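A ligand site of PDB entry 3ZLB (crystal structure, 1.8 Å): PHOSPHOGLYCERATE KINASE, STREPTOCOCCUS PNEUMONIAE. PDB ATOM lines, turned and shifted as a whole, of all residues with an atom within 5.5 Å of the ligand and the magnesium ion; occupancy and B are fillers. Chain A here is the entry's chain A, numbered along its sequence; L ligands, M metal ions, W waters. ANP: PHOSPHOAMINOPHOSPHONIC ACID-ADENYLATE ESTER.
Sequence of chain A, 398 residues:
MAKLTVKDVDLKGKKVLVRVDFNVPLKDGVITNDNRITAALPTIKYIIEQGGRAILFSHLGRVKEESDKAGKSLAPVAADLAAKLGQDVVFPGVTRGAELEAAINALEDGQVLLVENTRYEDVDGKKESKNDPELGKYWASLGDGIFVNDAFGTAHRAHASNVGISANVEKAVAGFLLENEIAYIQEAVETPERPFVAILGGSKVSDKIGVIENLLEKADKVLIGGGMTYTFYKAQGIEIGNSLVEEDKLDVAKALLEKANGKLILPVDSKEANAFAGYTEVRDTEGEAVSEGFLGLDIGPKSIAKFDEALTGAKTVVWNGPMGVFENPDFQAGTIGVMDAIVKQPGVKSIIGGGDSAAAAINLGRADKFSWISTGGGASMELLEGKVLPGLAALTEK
The magnesium ion is bound by water W12 (2.0 Å), O2A of the ligand (2.1 Å), O1B of the ligand (2.1 Å), O1G of the ligand (2.1 Å) and water W4 (2.1 Å).
The magnesium ion has five donor atoms within binding distance.
The side-chain carboxylate (OE2) of Glu 327 sits at hydrogen-bond distance from an oxygen (O3') of the ligand, at 2.6 Å.
O2B of the ligand sits at hydrogen-bond distance from N of Ser 357 (2.8 Å).
OG of Ser 357 sits at hydrogen-bond distance from O2B of the ligand (2.6 Å).
OD1 of Asn 320 is in hydrogen-bond range of N3B of the ligand (2.7 Å).
The backbone NH (N) of Gly 355 sits at hydrogen-bond distance from an oxygen (O2G) of the ligand (2.7 Å).
O2B of the ligand is in hydrogen-bond range of N of Asp 356, at 3.2 Å.
The backbone carbonyl oxygen (O) of Gly 296 is in hydrogen-bond range of a nitrogen (N6) of the ligand.
The side-chain amino group (NZ) of Lys 208 is in salt-bridge range of an oxygen (O1A) of the ligand (3.2 Å).
An oxygen (O4') of the ligand lies within hydrogen-bond range of the backbone NH (N) of Ser 203.
A nitrogen (N7) of the ligand lies within hydrogen-bond range of the backbone NH (N) of Gly 227, 3.3 Å away.
The side-chain hydroxyl of Ser 357 sits at hydrogen-bond distance from the backbone NH of Gly 321, 2.7 Å away.
O of Asn 320 is in hydrogen-bond range of N of Gly 201, at 2.9 Å.
The backbone carbonyl oxygen (O) of Gly 353 is in hydrogen-bond range of the side-chain amide nitrogen (ND2) of Asn 320 (3.1 Å).
The backbone NH (N) of Gly 202 sits at hydrogen-bond distance from the backbone carbonyl oxygen (O) of Pro 322, 2.8 Å away.
The backbone NH (N) of Gly 227 lies within hydrogen-bond range of the backbone carbonyl oxygen (O) of Gly 202, at 2.7 Å.
The side-chain carboxylate of Asp 207 is in salt-bridge range of the side-chain amino group of Lys 208 (3.7 Å).
The backbone NH (N) of Gly 226 lies within hydrogen-bond range of the backbone carbonyl oxygen (O) of Met 323.
The backbone carbonyl oxygen (O) of Leu 297 sits at hydrogen-bond distance from the backbone NH (N) of Val 325, at 2.9 Å.
The backbone carbonyl oxygen (O) of Gly 324 sits close to a nitrogen (N7) of the ligand (3.5 Å).
Merely in contact with the ligand: Gly 202, Gly 226, Tyr 230, Leu 244, Leu 297, Gly 321, Pro 322, Val 325, Gly 354 and Met 381.
Hydrophobic or aromatic side chains within 4 Å of the ligand: Tyr 230, Leu 244, Pro 322, Val 325 and Met 381.
20 residues have an atom within 4 Å of the ligand: Gly 202, Ser 203, Lys 208, Gly 226, Gly 227, Tyr 230, Leu 244, Gly 296, Leu 297, Asn 320, Gly 321, Pro 322, Gly 324, Val 325, Glu 327, Gly 354, Gly 355, Asp 356, Ser 357 and Met 381.
No residue comes within 4 Å of the magnesium ion.
Water W7 lies within hydrogen-bond range of an oxygen (O1A) of the ligand, the side-chain hydroxyl (OG) of Ser 203 and the side-chain carboxylate (OD1) of Asp 207.
Water W8 lies within hydrogen-bond range of O of Met 323 (2.8 Å), N6 of the ligand (2.8 Å) and N of Asp 298 (3.4 Å).
Water W10 lies within hydrogen-bond range of O of Gly 296 (2.8 Å), N1 of the ligand (2.9 Å) and N of Leu 244 (2.9 Å).
Water W9 bridges O3' of the ligand and OD2 of Asp 356.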
ATOM      1  N   GLY A 201      -7.218  -7.952  -6.962  1.00  0.00           N
ATOM      2  CA  GLY A 201      -6.738  -6.665  -7.415  1.00  0.00           C
ATOM      3  C   GLY A 201      -7.596  -6.112  -8.530  1.00  0.00           C
ATOM      4  O   GLY A 201      -8.826  -6.221  -8.490  1.00  0.00           O
ATOM      5  N   GLY A 202      -6.970  -5.480  -9.506  1.00  0.00           N
ATOM      6  CA  GLY A 202      -7.707  -4.859 -10.567  1.00  0.00           C
ATOM      7  C   GLY A 202      -8.206  -3.480 -10.205  1.00  0.00           C
ATOM      8  O   GLY A 202      -7.815  -2.900  -9.179  1.00  0.00           O
ATOM      9  N   SER A 203      -9.123  -2.958 -11.022  1.00  0.00           N
ATOM     10  CA  SER A 203      -9.474  -1.555 -11.022  1.00  0.00           C
ATOM     11  C   SER A 203     -10.457  -1.144  -9.905  1.00  0.00           C
ATOM     12  O   SER A 203     -10.357  -0.043  -9.379  1.00  0.00           O
ATOM     13  CB  SER A 203     -10.089  -1.164 -12.410  1.00  0.00           C
ATOM     14  OG  SER A 203     -11.062  -2.148 -12.834  1.00  0.00           O
ATOM     15  N   LYS A 204     -11.419  -2.016  -9.607  1.00  0.00           N
ATOM     16  CA  LYS A 204     -12.578  -1.644  -8.828  1.00  0.00           C
ATOM     17  C   LYS A 204     -13.140  -2.724  -7.894  1.00  0.00           C
ATOM     18  O   LYS A 204     -13.151  -3.917  -8.209  1.00  0.00           O
ATOM     19  CB  LYS A 204     -13.694  -1.199  -9.782  1.00  0.00           C
ATOM     20  CG  LYS A 204     -13.366   0.112 -10.456  1.00  0.00           C
ATOM     21  CD  LYS A 204     -14.429   0.512 -11.432  1.00  0.00           C
ATOM     22  CE  LYS A 204     -14.352  -0.316 -12.719  1.00  0.00           C
ATOM     23  NZ  LYS A 204     -15.470  -1.315 -12.832  1.00  0.00           N
ATOM     24  N   ASP A 207     -17.021  -4.809  -8.909  1.00  0.00           N
ATOM     25  CA  ASP A 207     -17.187  -6.066  -9.630  1.00  0.00           C
ATOM     26  C   ASP A 207     -16.643  -7.245  -8.835  1.00  0.00           C
ATOM     27  O   ASP A 207     -16.743  -8.391  -9.276  1.00  0.00           O
ATOM     28  CB  ASP A 207     -16.583  -6.023 -11.040  1.00  0.00           C
ATOM     29  CG  ASP A 207     -15.318  -5.218 -11.100  1.00  0.00           C
ATOM     30  OD1 ASP A 207     -14.392  -5.492 -10.305  1.00  0.00           O
ATOM     31  OD2 ASP A 207     -15.259  -4.292 -11.950  1.00  0.00           O
ATOM     32  N   LYS A 208     -16.101  -6.985  -7.643  1.00  0.00           N
ATOM     33  CA  LYS A 208     -15.538  -8.086  -6.842  1.00  0.00           C
ATOM     34  C   LYS A 208     -16.126  -8.259  -5.450  1.00  0.00           C
ATOM     35  O   LYS A 208     -15.633  -9.093  -4.668  1.00  0.00           O
ATOM     36  CB  LYS A 208     -14.035  -7.948  -6.780  1.00  0.00           C
ATOM     37  CG  LYS A 208     -13.340  -8.088  -8.132  1.00  0.00           C
ATOM     38  CD  LYS A 208     -11.958  -8.682  -7.971  1.00  0.00           C
ATOM     39  CE  LYS A 208     -10.993  -8.328  -9.114  1.00  0.00           C
ATOM     40  NZ  LYS A 208     -11.651  -7.903 -10.391  1.00  0.00           N
ATOM     41  N   GLY A 226      -4.252  -3.202  -6.362  1.00  0.00           N
ATOM     42  CA  GLY A 226      -4.837  -2.517  -7.495  1.00  0.00           C
ATOM     43  C   GLY A 226      -5.623  -1.295  -7.117  1.00  0.00           C
ATOM     44  O   GLY A 226      -5.445  -0.746  -6.007  1.00  0.00           O
ATOM     45  N   GLY A 227      -6.495  -0.844  -8.009  1.00  0.00           N
ATOM     46  CA  GLY A 227      -7.280   0.336  -7.758  1.00  0.00           C
ATOM     47  C   GLY A 227      -8.237   0.131  -6.618  1.00  0.00           C
ATOM     48  O   GLY A 227      -8.635   1.108  -5.983  1.00  0.00           O
ATOM     49  N   TYR A 230      -7.975   1.814  -3.067  1.00  0.00           N
ATOM     50  CA  TYR A 230      -8.177   3.227  -2.658  1.00  0.00           C
ATOM     51  C   TYR A 230      -9.591   3.449  -2.180  1.00  0.00           C
ATOM     52  O   TYR A 230      -9.860   4.387  -1.404  1.00  0.00           O
ATOM     53  CB  TYR A 230      -7.707   4.213  -3.754  1.00  0.00           C
ATOM     54  CG  TYR A 230      -6.309   3.878  -4.081  1.00  0.00           C
ATOM     55  CD1 TYR A 230      -5.282   4.183  -3.178  1.00  0.00           C
ATOM     56  CD2 TYR A 230      -5.985   3.114  -5.199  1.00  0.00           C
ATOM     57  CE1 TYR A 230      -3.971   3.779  -3.421  1.00  0.00           C
ATOM     58  CE2 TYR A 230      -4.672   2.701  -5.443  1.00  0.00           C
ATOM     59  CZ  TYR A 230      -3.680   3.050  -4.551  1.00  0.00           C
ATOM     60  OH  TYR A 230      -2.360   2.664  -4.752  1.00  0.00           O
ATOM     61  N   LEU A 244      -8.202   6.090  -8.266  1.00  0.00           N
ATOM     62  CA  LEU A 244      -9.485   5.557  -8.698  1.00  0.00           C
ATOM     63  C   LEU A 244     -10.254   5.088  -7.482  1.00  0.00           C
ATOM     64  O   LEU A 244      -9.762   4.248  -6.731  1.00  0.00           O
ATOM     65  CB  LEU A 244      -9.219   4.401  -9.633  1.00  0.00           C
ATOM     66  CG  LEU A 244     -10.337   3.919 -10.505  1.00  0.00           C
ATOM     67  CD1 LEU A 244     -10.849   5.091 -11.325  1.00  0.00           C
ATOM     68  CD2 LEU A 244      -9.775   2.815 -11.369  1.00  0.00           C
ATOM     69  N   PHE A 276      -1.892  10.344 -14.498  1.00  0.00           N
ATOM     70  CA  PHE A 276      -2.048   8.969 -14.919  1.00  0.00           C
ATOM     71  C   PHE A 276      -1.153   8.693 -16.120  1.00  0.00           C
ATOM     72  O   PHE A 276      -0.577   7.583 -16.255  1.00  0.00           O
ATOM     73  CB  PHE A 276      -3.509   8.668 -15.281  1.00  0.00           C
ATOM     74  CG  PHE A 276      -3.720   7.254 -15.750  1.00  0.00           C
ATOM     75  CD1 PHE A 276      -3.844   6.206 -14.846  1.00  0.00           C
ATOM     76  CD2 PHE A 276      -3.771   6.979 -17.107  1.00  0.00           C
ATOM     77  CE1 PHE A 276      -4.008   4.893 -15.269  1.00  0.00           C
ATOM     78  CE2 PHE A 276      -3.941   5.678 -17.558  1.00  0.00           C
ATOM     79  CZ  PHE A 276      -4.065   4.631 -16.654  1.00  0.00           C
ATOM     80  N   GLY A 296      -2.281   6.694  -6.751  1.00  0.00           N
ATOM     81  CA  GLY A 296      -1.565   5.444  -6.606  1.00  0.00           C
ATOM     82  C   GLY A 296      -1.752   4.540  -7.809  1.00  0.00           C
ATOM     83  O   GLY A 296      -2.888   4.295  -8.214  1.00  0.00           O
ATOM     84  N   LEU A 297      -0.650   4.035  -8.383  1.00  0.00           N
ATOM     85  CA  LEU A 297      -0.705   3.270  -9.636  1.00  0.00           C
ATOM     86  C   LEU A 297      -0.078   1.892  -9.505  1.00  0.00           C
ATOM     87  O   LEU A 297      -0.122   1.113 -10.447  1.00  0.00           O
ATOM     88  CB  LEU A 297      -0.045   4.022 -10.784  1.00  0.00           C
ATOM     89  CG  LEU A 297      -0.682   5.383 -11.088  1.00  0.00           C
ATOM     90  CD1 LEU A 297       0.182   6.173 -12.045  1.00  0.00           C
ATOM     91  CD2 LEU A 297      -2.121   5.234 -11.647  1.00  0.00           C
ATOM     92  N   ASP A 298       0.460   1.588  -8.341  1.00  0.00           N
ATOM     93  CA  ASP A 298       0.915   0.241  -8.043  1.00  0.00           C
ATOM     94  C   ASP A 298       1.017   0.099  -6.550  1.00  0.00           C
ATOM     95  O   ASP A 298       1.101   1.101  -5.820  1.00  0.00           O
ATOM     96  CB  ASP A 298       2.279  -0.010  -8.700  1.00  0.00           C
ATOM     97  CG  ASP A 298       2.610  -1.500  -8.851  1.00  0.00           C
ATOM     98  OD1 ASP A 298       1.741  -2.361  -8.532  1.00  0.00           O
ATOM     99  OD2 ASP A 298       3.743  -1.819  -9.285  1.00  0.00           O
ATOM    100  N   ASN A 320      -7.044 -12.986  -8.710  1.00  0.00           N
ATOM    101  CA  ASN A 320      -7.673 -12.240  -9.779  1.00  0.00           C
ATOM    102  C   ASN A 320      -7.432 -10.763  -9.590  1.00  0.00           C
ATOM    103  O   ASN A 320      -7.987 -10.159  -8.666  1.00  0.00           O
ATOM    104  CB  ASN A 320      -9.173 -12.494  -9.835  1.00  0.00           C
ATOM    105  CG  ASN A 320      -9.867 -11.670 -10.908  1.00  0.00           C
ATOM    106  OD1 ASN A 320      -9.267 -10.805 -11.538  1.00  0.00           O
ATOM    107  ND2 ASN A 320     -11.166 -11.892 -11.077  1.00  0.00           N
ATOM    108  N   GLY A 321      -6.614 -10.178 -10.454  1.00  0.00           N
ATOM    109  CA  GLY A 321      -6.549  -8.739 -10.612  1.00  0.00           C
ATOM    110  C   GLY A 321      -5.146  -8.187 -10.416  1.00  0.00           C
ATOM    111  O   GLY A 321      -4.516  -8.453  -9.401  1.00  0.00           O
ATOM    112  N   PRO A 322      -4.653  -7.423 -11.401  1.00  0.00           N
ATOM    113  CA  PRO A 322      -3.296  -6.900 -11.233  1.00  0.00           C
ATOM    114  C   PRO A 322      -3.171  -5.968 -10.050  1.00  0.00           C
ATOM    115  O   PRO A 322      -4.188  -5.340  -9.644  1.00  0.00           O
ATOM    116  CB  PRO A 322      -3.064  -6.128 -12.539  1.00  0.00           C
ATOM    117  CG  PRO A 322      -3.955  -6.858 -13.561  1.00  0.00           C
ATOM    118  CD  PRO A 322      -5.195  -7.197 -12.747  1.00  0.00           C
ATOM    119  N   MET A 323      -1.962  -5.886  -9.480  1.00  0.00           N
ATOM    120  CA  MET A 323      -1.696  -5.082  -8.300  1.00  0.00           C
ATOM    121  C   MET A 323      -1.507  -3.615  -8.613  1.00  0.00           C
ATOM    122  O   MET A 323      -1.482  -2.784  -7.703  1.00  0.00           O
ATOM    123  CB  MET A 323      -0.429  -5.583  -7.595  1.00  0.00           C
ATOM    124  CG  MET A 323      -0.546  -6.998  -7.011  1.00  0.00           C
ATOM    125  SD  MET A 323      -1.686  -7.179  -5.611  1.00  0.00           S
ATOM    126  CE  MET A 323      -3.203  -7.716  -6.441  1.00  0.00           C
ATOM    127  N   GLY A 324      -1.367  -3.310  -9.913  1.00  0.00           N
ATOM    128  CA  GLY A 324      -1.116  -1.959 -10.380  1.00  0.00           C
ATOM    129  C   GLY A 324      -1.430  -1.838 -11.858  1.00  0.00           C
ATOM    130  O   GLY A 324      -1.965  -2.765 -12.462  1.00  0.00           O
ATOM    131  N   VAL A 325      -1.129  -0.695 -12.448  1.00  0.00           N
ATOM    132  CA  VAL A 325      -1.446  -0.438 -13.859  1.00  0.00           C
ATOM    133  C   VAL A 325      -0.414  -1.155 -14.745  1.00  0.00           C
ATOM    134  O   VAL A 325       0.557  -0.579 -15.213  1.00  0.00           O
ATOM    135  CB  VAL A 325      -1.453   1.079 -14.101  1.00  0.00           C
ATOM    136  CG1 VAL A 325      -1.682   1.411 -15.565  1.00  0.00           C
ATOM    137  CG2 VAL A 325      -2.532   1.709 -13.210  1.00  0.00           C
ATOM    138  N   PHE A 326      -0.659  -2.443 -14.941  1.00  0.00           N
ATOM    139  CA  PHE A 326       0.315  -3.357 -15.478  1.00  0.00           C
ATOM    140  C   PHE A 326       0.637  -3.081 -16.936  1.00  0.00           C
ATOM    141  O   PHE A 326       1.669  -3.509 -17.452  1.00  0.00           O
ATOM    142  CB  PHE A 326      -0.236  -4.750 -15.344  1.00  0.00           C
ATOM    143  CG  PHE A 326       0.758  -5.787 -15.594  1.00  0.00           C
ATOM    144  CD1 PHE A 326       1.568  -6.236 -14.562  1.00  0.00           C
ATOM    145  CD2 PHE A 326       0.928  -6.287 -16.863  1.00  0.00           C
ATOM    146  CE1 PHE A 326       2.525  -7.212 -14.799  1.00  0.00           C
ATOM    147  CE2 PHE A 326       1.875  -7.241 -17.127  1.00  0.00           C
ATOM    148  CZ  PHE A 326       2.681  -7.711 -16.097  1.00  0.00           C
ATOM    149  N   GLU A 327      -0.271  -2.369 -17.610  1.00  0.00           N
ATOM    150  CA  GLU A 327      -0.078  -1.992 -19.009  1.00  0.00           C
ATOM    151  C   GLU A 327       1.188  -1.143 -19.146  1.00  0.00           C
ATOM    152  O   GLU A 327       1.793  -1.070 -20.207  1.00  0.00           O
ATOM    153  CB  GLU A 327      -1.265  -1.166 -19.502  1.00  0.00           C
ATOM    154  CG  GLU A 327      -2.599  -1.884 -19.584  1.00  0.00           C
ATOM    155  CD  GLU A 327      -3.450  -1.740 -18.334  1.00  0.00           C
ATOM    156  OE1 GLU A 327      -2.898  -1.636 -17.203  1.00  0.00           O
ATOM    157  OE2 GLU A 327      -4.702  -1.723 -18.470  1.00  0.00           O
ATOM    158  N   GLY A 353      -7.568 -16.370 -12.129  1.00  0.00           N
ATOM    159  CA  GLY A 353      -8.918 -16.231 -12.614  1.00  0.00           C
ATOM    160  C   GLY A 353      -9.325 -14.831 -13.033  1.00  0.00           C
ATOM    161  O   GLY A 353     -10.439 -14.403 -12.730  1.00  0.00           O
ATOM    162  N   GLY A 354      -8.474 -14.142 -13.766  1.00  0.00           N
ATOM    163  CA  GLY A 354      -8.830 -12.866 -14.369  1.00  0.00           C
ATOM    164  C   GLY A 354      -8.116 -12.704 -15.677  1.00  0.00           C
ATOM    165  O   GLY A 354      -7.067 -13.311 -15.892  1.00  0.00           O
ATOM    166  N   GLY A 355      -8.701 -11.917 -16.585  1.00  0.00           N
ATOM    167  CA  GLY A 355      -8.202 -11.745 -17.936  1.00  0.00           C
ATOM    168  C   GLY A 355      -6.875 -11.036 -18.077  1.00  0.00           C
ATOM    169  O   GLY A 355      -5.958 -11.547 -18.740  1.00  0.00           O
ATOM    170  N   ASP A 356      -6.767  -9.838 -17.488  1.00  0.00           N
ATOM    171  CA  ASP A 356      -5.508  -9.099 -17.475  1.00  0.00           C
ATOM    172  C   ASP A 356      -4.495  -9.830 -16.624  1.00  0.00           C
ATOM    173  O   ASP A 356      -3.292  -9.773 -16.910  1.00  0.00           O
ATOM    174  CB  ASP A 356      -5.719  -7.706 -16.884  1.00  0.00           C
ATOM    175  CG  ASP A 356      -6.123  -6.681 -17.918  1.00  0.00           C
ATOM    176  OD1 ASP A 356      -6.552  -7.057 -19.036  1.00  0.00           O
ATOM    177  OD2 ASP A 356      -5.979  -5.480 -17.618  1.00  0.00           O
ATOM    178  N   SER A 357      -4.957 -10.508 -15.593  1.00  0.00           N
ATOM    179  CA  SER A 357      -4.031 -11.256 -14.723  1.00  0.00           C
ATOM    180  C   SER A 357      -3.353 -12.407 -15.485  1.00  0.00           C
ATOM    181  O   SER A 357      -2.135 -12.606 -15.388  1.00  0.00           O
ATOM    182  CB  SER A 357      -4.774 -11.811 -13.510  1.00  0.00           C
ATOM    183  OG  SER A 357      -5.468 -10.771 -12.810  1.00  0.00           O
ATOM    184  N   ALA A 358      -4.137 -13.171 -16.241  1.00  0.00           N
ATOM    185  CA  ALA A 358      -3.550 -14.243 -17.063  1.00  0.00           C
ATOM    186  C   ALA A 358      -2.625 -13.652 -18.112  1.00  0.00           C
ATOM    187  O   ALA A 358      -1.543 -14.164 -18.340  1.00  0.00           O
ATOM    188  CB  ALA A 358      -4.652 -15.070 -17.716  1.00  0.00           C
ATOM    189  N   MET A 381     -15.822 -15.807 -12.258  1.00  0.00           N
ATOM    190  CA  MET A 381     -16.231 -14.878 -11.201  1.00  0.00           C
ATOM    191  C   MET A 381     -17.417 -15.414 -10.438  1.00  0.00           C
ATOM    192  O   MET A 381     -17.416 -15.404  -9.219  1.00  0.00           O
ATOM    193  CB  MET A 381     -16.599 -13.530 -11.824  1.00  0.00           C
ATOM    194  CG  MET A 381     -17.064 -12.436 -10.852  1.00  0.00           C
ATOM    195  SD  MET A 381     -15.743 -11.809  -9.805  1.00  0.00           S
ATOM    196  CE  MET A 381     -14.278 -12.297 -10.706  1.00  0.00           C
HETATM  197  PG  ANP L   1     -11.336  -9.759 -14.624  1.00  0.00           P
HETATM  198  O1G ANP L   1     -11.696  -8.529 -15.415  1.00  0.00           O
HETATM  199  O2G ANP L   1     -11.062 -10.956 -15.615  1.00  0.00           O
HETATM  200  O3G ANP L   1     -12.370 -10.172 -13.499  1.00  0.00           O
HETATM  201  PB  ANP L   1      -8.574  -8.730 -14.510  1.00  0.00           P
HETATM  202  O1B ANP L   1      -8.856  -8.425 -15.960  1.00  0.00           O
HETATM  203  O2B ANP L   1      -7.271  -9.541 -14.304  1.00  0.00           O
HETATM  204  N3B ANP L   1      -9.905  -9.452 -13.751  1.00  0.00           N
HETATM  205  PA  ANP L   1      -9.381  -6.119 -13.778  1.00  0.00           P
HETATM  206  O1A ANP L   1     -10.303  -6.085 -12.624  1.00  0.00           O
HETATM  207  O2A ANP L   1     -10.059  -6.003 -15.131  1.00  0.00           O
HETATM  208  O3A ANP L   1      -8.347  -7.354 -13.763  1.00  0.00           O
HETATM  209  O5' ANP L   1      -8.424  -4.878 -13.616  1.00  0.00           O
HETATM  210  C5' ANP L   1      -7.436  -4.626 -14.602  1.00  0.00           C
HETATM  211  C4' ANP L   1      -7.287  -3.139 -14.715  1.00  0.00           C
HETATM  212  O4' ANP L   1      -6.963  -2.632 -13.405  1.00  0.00           O
HETATM  213  C3' ANP L   1      -6.159  -2.667 -15.641  1.00  0.00           C
HETATM  214  O3' ANP L   1      -6.649  -1.853 -16.689  1.00  0.00           O
HETATM  215  C2' ANP L   1      -5.231  -1.872 -14.696  1.00  0.00           C
HETATM  216  O2' ANP L   1      -4.619  -0.716 -15.283  1.00  0.00           O
HETATM  217  C1' ANP L   1      -6.217  -1.465 -13.621  1.00  0.00           C
HETATM  218  N9  ANP L   1      -5.557  -1.015 -12.360  1.00  0.00           N
HETATM  219  C8  ANP L   1      -4.786  -1.780 -11.523  1.00  0.00           C
HETATM  220  N7  ANP L   1      -4.310  -1.068 -10.522  1.00  0.00           N
HETATM  221  C5  ANP L   1      -4.776   0.208 -10.716  1.00  0.00           C
HETATM  222  C6  ANP L   1      -4.646   1.404 -10.009  1.00  0.00           C
HETATM  223  N6  ANP L   1      -3.921   1.525  -8.877  1.00  0.00           N
HETATM  224  N1  ANP L   1      -5.274   2.509 -10.476  1.00  0.00           N
HETATM  225  C2  ANP L   1      -5.983   2.403 -11.609  1.00  0.00           C
HETATM  226  N3  ANP L   1      -6.213   1.322 -12.360  1.00  0.00           N
HETATM  227  C4  ANP L   1      -5.584   0.257 -11.878  1.00  0.00           C
HETATM  228 MG    MG M   1     -10.488  -7.349 -16.631  1.00  0.00          MG
HETATM  229  O   HOH W   1      -7.114   2.043 -15.033  1.00  0.00           O
HETATM  230  O   HOH W   2     -11.136  -5.337  -9.760  1.00  0.00           O
HETATM  231  O   HOH W   3     -13.151  -6.318 -13.889  1.00  0.00           O
HETATM  232  O   HOH W   4     -10.830  -8.547 -18.316  1.00  0.00           O
HETATM  233  O   HOH W   5     -12.252 -11.011 -17.869  1.00  0.00           O
HETATM  234  O   HOH W   6     -10.955  -3.129 -15.575  1.00  0.00           O
HETATM  235  O   HOH W   7     -12.414  -4.464 -12.062  1.00  0.00           O
HETATM  236  O   HOH W   8      -2.243  -0.109  -7.305  1.00  0.00           O
HETATM  237  O   HOH W   9      -8.838  -3.526 -17.775  1.00  0.00           O
HETATM  238  O   HOH W  10      -5.588   4.887  -8.850  1.00  0.00           O
HETATM  239  O   HOH W  11     -13.622 -12.371 -14.035  1.00  0.00           O
HETATM  240  O   HOH W  12      -9.278  -6.191 -17.779  1.00  0.00           O
